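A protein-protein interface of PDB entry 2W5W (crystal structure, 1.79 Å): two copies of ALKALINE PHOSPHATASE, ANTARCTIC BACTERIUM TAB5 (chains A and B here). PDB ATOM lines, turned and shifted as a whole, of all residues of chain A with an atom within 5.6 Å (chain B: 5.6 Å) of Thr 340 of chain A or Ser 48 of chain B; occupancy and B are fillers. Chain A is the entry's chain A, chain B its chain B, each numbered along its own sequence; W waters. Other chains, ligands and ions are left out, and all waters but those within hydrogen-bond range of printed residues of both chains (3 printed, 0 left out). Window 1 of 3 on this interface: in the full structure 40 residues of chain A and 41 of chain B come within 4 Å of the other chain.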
ATOM      1  N   GLY A  46      15.789 -15.533  29.689  1.00  0.00           N
ATOM      2  CA  GLY A  46      16.818 -14.656  30.205  1.00  0.00           C
ATOM      3  C   GLY A  46      16.183 -13.341  30.622  1.00  0.00           C
ATOM      4  O   GLY A  46      14.965 -13.178  30.584  1.00  0.00           O
ATOM      5  N   ILE A  72      22.751 -16.496  38.242  1.00  0.00           N
ATOM      6  CA  ILE A  72      23.388 -17.799  38.136  1.00  0.00           C
ATOM      7  C   ILE A  72      24.092 -18.029  36.798  1.00  0.00           C
ATOM      8  O   ILE A  72      23.612 -17.624  35.734  1.00  0.00           O
ATOM      9  CB  ILE A  72      22.414 -18.990  38.395  1.00  0.00           C
ATOM     10  CG1 ILE A  72      21.125 -18.850  37.579  1.00  0.00           C
ATOM     11  CG2 ILE A  72      22.075 -19.095  39.880  1.00  0.00           C
ATOM     12  CD1 ILE A  72      20.229 -20.129  37.642  1.00  0.00           C
ATOM     13  N   THR A  74      25.130 -20.836  34.137  1.00  0.00           N
ATOM     14  CA  THR A  74      24.355 -22.028  33.800  1.00  0.00           C
ATOM     15  C   THR A  74      25.092 -23.128  33.017  1.00  0.00           C
ATOM     16  O   THR A  74      24.478 -24.131  32.654  1.00  0.00           O
ATOM     17  CB  THR A  74      23.099 -21.639  33.000  1.00  0.00           C
ATOM     18  OG1 THR A  74      23.503 -21.039  31.763  1.00  0.00           O
ATOM     19  CG2 THR A  74      22.248 -20.629  33.790  1.00  0.00           C
ATOM     20  N   HIS A 302      18.183 -21.370  31.586  1.00  0.00           N
ATOM     21  CA  HIS A 302      19.084 -20.748  30.583  1.00  0.00           C
ATOM     22  C   HIS A 302      18.210 -19.827  29.734  1.00  0.00           C
ATOM     23  O   HIS A 302      16.996 -19.783  29.914  1.00  0.00           O
ATOM     24  CB  HIS A 302      19.681 -21.817  29.657  1.00  0.00           C
ATOM     25  CG  HIS A 302      18.626 -22.644  28.997  1.00  0.00           C
ATOM     26  ND1 HIS A 302      17.940 -22.227  27.871  1.00  0.00           N
ATOM     27  CD2 HIS A 302      18.053 -23.811  29.368  1.00  0.00           C
ATOM     28  CE1 HIS A 302      17.012 -23.117  27.571  1.00  0.00           C
ATOM     29  NE2 HIS A 302      17.065 -24.092  28.462  1.00  0.00           N
ATOM     30  N   GLU A 303      18.826 -19.102  28.806  1.00  0.00           N
ATOM     31  CA  GLU A 303      18.116 -18.213  27.895  1.00  0.00           C
ATOM     32  C   GLU A 303      17.976 -18.964  26.588  1.00  0.00           C
ATOM     33  O   GLU A 303      18.794 -19.836  26.291  1.00  0.00           O
ATOM     34  CB  GLU A 303      18.989 -16.980  27.616  1.00  0.00           C
ATOM     35  CG  GLU A 303      18.291 -15.813  26.911  1.00  0.00           C
ATOM     36  CD  GLU A 303      18.311 -15.886  25.385  1.00  0.00           C
ATOM     37  OE1 GLU A 303      19.154 -16.602  24.796  1.00  0.00           O
ATOM     38  OE2 GLU A 303      17.487 -15.176  24.769  1.00  0.00           O
ATOM     39  N   SER A 338      21.339 -20.053  24.940  1.00  0.00           N
ATOM     40  CA  SER A 338      22.565 -19.265  25.093  1.00  0.00           C
ATOM     41  C   SER A 338      23.070 -19.293  26.538  1.00  0.00           C
ATOM     42  O   SER A 338      22.330 -19.671  27.452  1.00  0.00           O
ATOM     43  CB  SER A 338      22.371 -17.814  24.603  1.00  0.00           C
ATOM     44  OG  SER A 338      21.563 -17.045  25.490  1.00  0.00           O
ATOM     45  N   ALA A 339      24.314 -18.857  26.740  1.00  0.00           N
ATOM     46  CA  ALA A 339      24.991 -19.013  28.026  1.00  0.00           C
ATOM     47  C   ALA A 339      25.027 -17.763  28.912  1.00  0.00           C
ATOM     48  O   ALA A 339      25.836 -17.687  29.830  1.00  0.00           O
ATOM     49  CB  ALA A 339      26.409 -19.521  27.809  1.00  0.00           C
ATOM     50  N   THR A 340      24.156 -16.797  28.661  1.00  0.00           N
ATOM     51  CA  THR A 340      24.079 -15.634  29.553  1.00  0.00           C
ATOM     52  C   THR A 340      23.806 -16.076  30.996  1.00  0.00           C
ATOM     53  O   THR A 340      23.136 -17.097  31.226  1.00  0.00           O
ATOM     54  CB  THR A 340      22.993 -14.649  29.107  1.00  0.00           C
ATOM     55  OG1 THR A 340      22.961 -13.518  30.004  1.00  0.00           O
ATOM     56  CG2 THR A 340      21.624 -15.328  29.089  1.00  0.00           C
ATOM     57  N   LEU A 341      24.336 -15.326  31.962  1.00  0.00           N
ATOM     58  CA  LEU A 341      23.898 -15.467  33.345  1.00  0.00           C
ATOM     59  C   LEU A 341      22.396 -15.229  33.393  1.00  0.00           C
ATOM     60  O   LEU A 341      21.856 -14.486  32.567  1.00  0.00           O
ATOM     61  CB  LEU A 341      24.579 -14.436  34.247  1.00  0.00           C
ATOM     62  CG  LEU A 341      26.075 -14.572  34.502  1.00  0.00           C
ATOM     63  CD1 LEU A 341      26.526 -13.500  35.495  1.00  0.00           C
ATOM     64  CD2 LEU A 341      26.393 -15.933  35.017  1.00  0.00           C
ATOM     65  N   ILE A 342      21.739 -15.830  34.380  1.00  0.00           N
ATOM     66  CA  ILE A 342      20.291 -15.800  34.519  1.00  0.00           C
ATOM     67  C   ILE A 342      19.896 -15.206  35.880  1.00  0.00           C
ATOM     68  O   ILE A 342      20.474 -15.553  36.907  1.00  0.00           O
ATOM     69  CB  ILE A 342      19.739 -17.239  34.428  1.00  0.00           C
ATOM     70  CG1 ILE A 342      19.939 -17.799  33.016  1.00  0.00           C
ATOM     71  CG2 ILE A 342      18.266 -17.302  34.899  1.00  0.00           C
ATOM     72  CD1 ILE A 342      19.144 -17.080  31.908  1.00  0.00           C
ATOM     73  N   GLY B  46      24.156  -5.000  28.481  1.00  0.00           N
ATOM     74  CA  GLY B  46      23.113  -5.764  29.144  1.00  0.00           C
ATOM     75  C   GLY B  46      23.708  -6.946  29.895  1.00  0.00           C
ATOM     76  O   GLY B  46      24.925  -7.134  29.932  1.00  0.00           O
ATOM     77  N   LEU B  47      22.860  -7.771  30.486  1.00  0.00           N
ATOM     78  CA  LEU B  47      23.377  -8.933  31.209  1.00  0.00           C
ATOM     79  C   LEU B  47      24.151  -9.908  30.289  1.00  0.00           C
ATOM     80  O   LEU B  47      25.121 -10.533  30.717  1.00  0.00           O
ATOM     81  CB  LEU B  47      22.236  -9.641  31.945  1.00  0.00           C
ATOM     82  CG  LEU B  47      22.580 -10.858  32.801  1.00  0.00           C
ATOM     83  CD1 LEU B  47      23.670 -10.535  33.837  1.00  0.00           C
ATOM     84  CD2 LEU B  47      21.284 -11.342  33.498  1.00  0.00           C
ATOM     85  N   SER B  48      23.764 -10.031  29.020  1.00  0.00           N
ATOM     86  CA  SER B  48      24.554 -10.880  28.117  1.00  0.00           C
ATOM     87  C   SER B  48      25.989 -10.366  27.927  1.00  0.00           C
ATOM     88  O   SER B  48      26.951 -11.145  27.930  1.00  0.00           O
ATOM     89  CB  SER B  48      23.856 -11.046  26.759  1.00  0.00           C
ATOM     90  OG  SER B  48      22.607 -11.718  26.900  1.00  0.00           O
ATOM     91  N   GLN B  49      26.146  -9.057  27.786  1.00  0.00           N
ATOM     92  CA  GLN B  49      27.481  -8.478  27.682  1.00  0.00           C
ATOM     93  C   GLN B  49      28.281  -8.708  28.967  1.00  0.00           C
ATOM     94  O   GLN B  49      29.448  -9.111  28.919  1.00  0.00           O
ATOM     95  CB  GLN B  49      27.416  -6.971  27.376  1.00  0.00           C
ATOM     96  CG  GLN B  49      27.058  -6.604  25.944  1.00  0.00           C
ATOM     97  CD  GLN B  49      25.562  -6.540  25.689  1.00  0.00           C
ATOM     98  OE1 GLN B  49      24.767  -7.007  26.499  1.00  0.00           O
ATOM     99  NE2 GLN B  49      25.175  -5.956  24.557  1.00  0.00           N
ATOM    100  N   ILE B  50      27.652  -8.448  30.111  1.00  0.00           N
ATOM    101  CA  ILE B  50      28.287  -8.701  31.406  1.00  0.00           C
ATOM    102  C   ILE B  50      28.734 -10.161  31.483  1.00  0.00           C
ATOM    103  O   ILE B  50      29.842 -10.472  31.929  1.00  0.00           O
ATOM    104  CB  ILE B  50      27.313  -8.390  32.566  1.00  0.00           C
ATOM    105  CG1 ILE B  50      27.056  -6.873  32.655  1.00  0.00           C
ATOM    106  CG2 ILE B  50      27.848  -8.967  33.900  1.00  0.00           C
ATOM    107  CD1 ILE B  50      25.819  -6.521  33.522  1.00  0.00           C
ATOM    108  N   SER B  51      27.879 -11.060  31.011  1.00  0.00           N
ATOM    109  CA  SER B  51      28.171 -12.495  31.083  1.00  0.00           C
ATOM    110  C   SER B  51      29.411 -12.909  30.295  1.00  0.00           C
ATOM    111  O   SER B  51      30.037 -13.913  30.610  1.00  0.00           O
ATOM    112  CB  SER B  51      26.967 -13.304  30.624  1.00  0.00           C
ATOM    113  OG  SER B  51      25.854 -13.001  31.438  1.00  0.00           O
ATOM    114  N   SER B  52      29.794 -12.133  29.286  1.00  0.00           N
ATOM    115  CA  SER B  52      30.929 -12.547  28.473  1.00  0.00           C
ATOM    116  C   SER B  52      32.212 -12.544  29.301  1.00  0.00           C
ATOM    117  O   SER B  52      33.158 -13.278  28.992  1.00  0.00           O
ATOM    118  CB  SER B  52      31.068 -11.661  27.223  1.00  0.00           C
ATOM    119  OG  SER B  52      31.422 -10.340  27.568  1.00  0.00           O
ATOM    120  N   TYR B  55      33.261 -15.929  30.553  1.00  0.00           N
ATOM    121  CA  TYR B  55      33.717 -16.925  29.575  1.00  0.00           C
ATOM    122  C   TYR B  55      34.962 -16.499  28.800  1.00  0.00           C
ATOM    123  O   TYR B  55      35.728 -17.339  28.311  1.00  0.00           O
ATOM    124  CB  TYR B  55      32.581 -17.219  28.590  1.00  0.00           C
ATOM    125  CG  TYR B  55      31.421 -17.906  29.261  1.00  0.00           C
ATOM    126  CD1 TYR B  55      30.368 -17.174  29.805  1.00  0.00           C
ATOM    127  CD2 TYR B  55      31.397 -19.290  29.388  1.00  0.00           C
ATOM    128  CE1 TYR B  55      29.316 -17.797  30.433  1.00  0.00           C
ATOM    129  CE2 TYR B  55      30.350 -19.924  30.017  1.00  0.00           C
ATOM    130  CZ  TYR B  55      29.315 -19.176  30.541  1.00  0.00           C
ATOM    131  OH  TYR B  55      28.272 -19.794  31.168  1.00  0.00           O
ATOM    132  N   PHE B 307      23.371  -8.705  21.777  1.00  0.00           N
ATOM    133  CA  PHE B 307      24.522  -9.586  21.962  1.00  0.00           C
ATOM    134  C   PHE B 307      24.077 -10.855  22.684  1.00  0.00           C
ATOM    135  O   PHE B 307      23.369 -10.798  23.703  1.00  0.00           O
ATOM    136  CB  PHE B 307      25.604  -8.847  22.767  1.00  0.00           C
ATOM    137  CG  PHE B 307      26.821  -9.679  23.087  1.00  0.00           C
ATOM    138  CD1 PHE B 307      27.802  -9.907  22.133  1.00  0.00           C
ATOM    139  CD2 PHE B 307      27.001 -10.203  24.358  1.00  0.00           C
ATOM    140  CE1 PHE B 307      28.935 -10.660  22.432  1.00  0.00           C
ATOM    141  CE2 PHE B 307      28.138 -10.968  24.675  1.00  0.00           C
ATOM    142  CZ  PHE B 307      29.109 -11.193  23.710  1.00  0.00           C
ATOM    143  N   THR B 308      24.486 -11.999  22.149  1.00  0.00           N
ATOM    144  CA  THR B 308      24.005 -13.290  22.646  1.00  0.00           C
ATOM    145  C   THR B 308      25.143 -14.305  22.689  1.00  0.00           C
ATOM    146  O   THR B 308      25.901 -14.434  21.728  1.00  0.00           O
ATOM    147  CB  THR B 308      22.886 -13.792  21.729  1.00  0.00           C
ATOM    148  OG1 THR B 308      21.823 -12.831  21.746  1.00  0.00           O
ATOM    149  CG2 THR B 308      22.337 -15.151  22.194  1.00  0.00           C
ATOM    150  N   LEU B 309      25.266 -15.014  23.807  1.00  0.00           N
ATOM    151  CA  LEU B 309      26.301 -16.036  23.952  1.00  0.00           C
ATOM    152  C   LEU B 309      25.761 -17.374  23.419  1.00  0.00           C
ATOM    153  O   LEU B 309      25.582 -18.348  24.158  1.00  0.00           O
ATOM    154  CB  LEU B 309      26.755 -16.140  25.417  1.00  0.00           C
ATOM    155  CG  LEU B 309      27.390 -14.860  25.976  1.00  0.00           C
ATOM    156  CD1 LEU B 309      27.697 -15.024  27.460  1.00  0.00           C
ATOM    157  CD2 LEU B 309      28.653 -14.471  25.210  1.00  0.00           C
HETATM  158  O   HOH W   1      23.124 -14.755  25.833  1.00  0.00           O
HETATM  159  O   HOH W   2      20.590 -11.600  28.996  1.00  0.00           O
HETATM  160  O   HOH W   3      25.886 -18.692  32.400  1.00  0.00           O
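Hydrophobic or aromatic side chains of chain A that line the printed part of chain B: Ala 339 and Leu 341. Of the 11 printed residues of chain B, 6 touch a printed residue of chain A. Among the printed residues, 9 pairs touch across the chains.
Ser 338 of chain A touches Thr 308 of chain B (CB to CG2, 3.6 Å). Leu 309 of chain B touches Ser 338 of chain A. Leu 47 of chain B touches Thr 340 of chain A. Ser 48 of chain B touches Thr 340 of chain A. Leu 341 of chain A touches Leu 47 of chain B (O to CD2, 3.3 Å).
Water W3 lies within hydrogen-bond range of the backbone carbonyl oxygen (O) of Ala 339 of chain A (2.8 Å), the backbone NH (N) of Thr 74 of chain A (2.9 Å), the side-chain hydroxyl (OH) of Tyr 55 of chain B (2.9 Å) and the backbone carbonyl oxygen (O) of Thr 340 of chain A (3.4 Å). Water W1 lies within hydrogen-bond range of OG of Ser 338 of chain A (2.8 Å), N of Leu 309 of chain B (3.0 Å) and OG of Ser 48 of chain B (3.3 Å). Water W2 lies within hydrogen-bond range of the side-chain hydroxyl of Ser 48 of chain B (2.9 Å) and the side-chain hydroxyl of Thr 340 of chain A (3.2 Å).
1 position is printed for both chains. Of the 9 pairs that touch across the chains among the printed residues, none has its exchanged pair printed and touching as well.
The side-chain hydroxyl of Tyr 55 of chain B is in hydrogen-bond range of the backbone carbonyl oxygen of Ala 339 of chain A. N of Ala 339 of chain A is in hydrogen-bond range of O of Leu 309 of chain B (2.9 Å). OG1 of Thr 340 of chain A lies within hydrogen-bond range of OG of Ser 51 of chain B (3.3 Å). The backbone NH of Leu 341 of chain A sits at hydrogen-bond distance from the side-chain hydroxyl of Ser 51 of chain B (2.8 Å).
The side-chain carboxylate (OE1) of Glu 303 of chain A lies within hydrogen-bond range of the side-chain hydroxyl (OG) of Ser 338 of chain A, at 2.5 Å. O of Leu 47 of chain B sits at hydrogen-bond distance from OG of Ser 51 of chain B, 2.7 Å away. OG of Ser 48 of chain B sits close to O of Phe 307 of chain B.
Of chain A, only Thr 340 (3.6 Å) comes within 4 Å of Ser 48 of chain B. Of the printed residues of chain B, Ala 339 of chain A touches Tyr 55 (3.5 Å) and Leu 309 (2.9 Å). Of the printed residues of chain A, Leu 309 of chain B touches Ser 338 (3.3 Å) and Ala 339 (2.9 Å). Of the printed residues of chain A, Ser 51 of chain B touches Thr 340 and Leu 341. Of the printed residues of chain A, Leu 47 of chain B touches Thr 340 and Leu 341. Printed residues of chain A within 4 Å of Tyr 55 of chain B: Ala 339 (3.5 Å). The nearest residue of chain B that does not touch Thr 340 of chain A is Leu 309 of chain B (4.1 Å). The nearest printed residue of chain A that does not touch Ser 48 of chain B is Ser 338 of chain A (5.6 Å). The nearest printed residue of chain B that does not touch Ser 338 of chain A is Ser 48 of chain B (5.6 Å).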
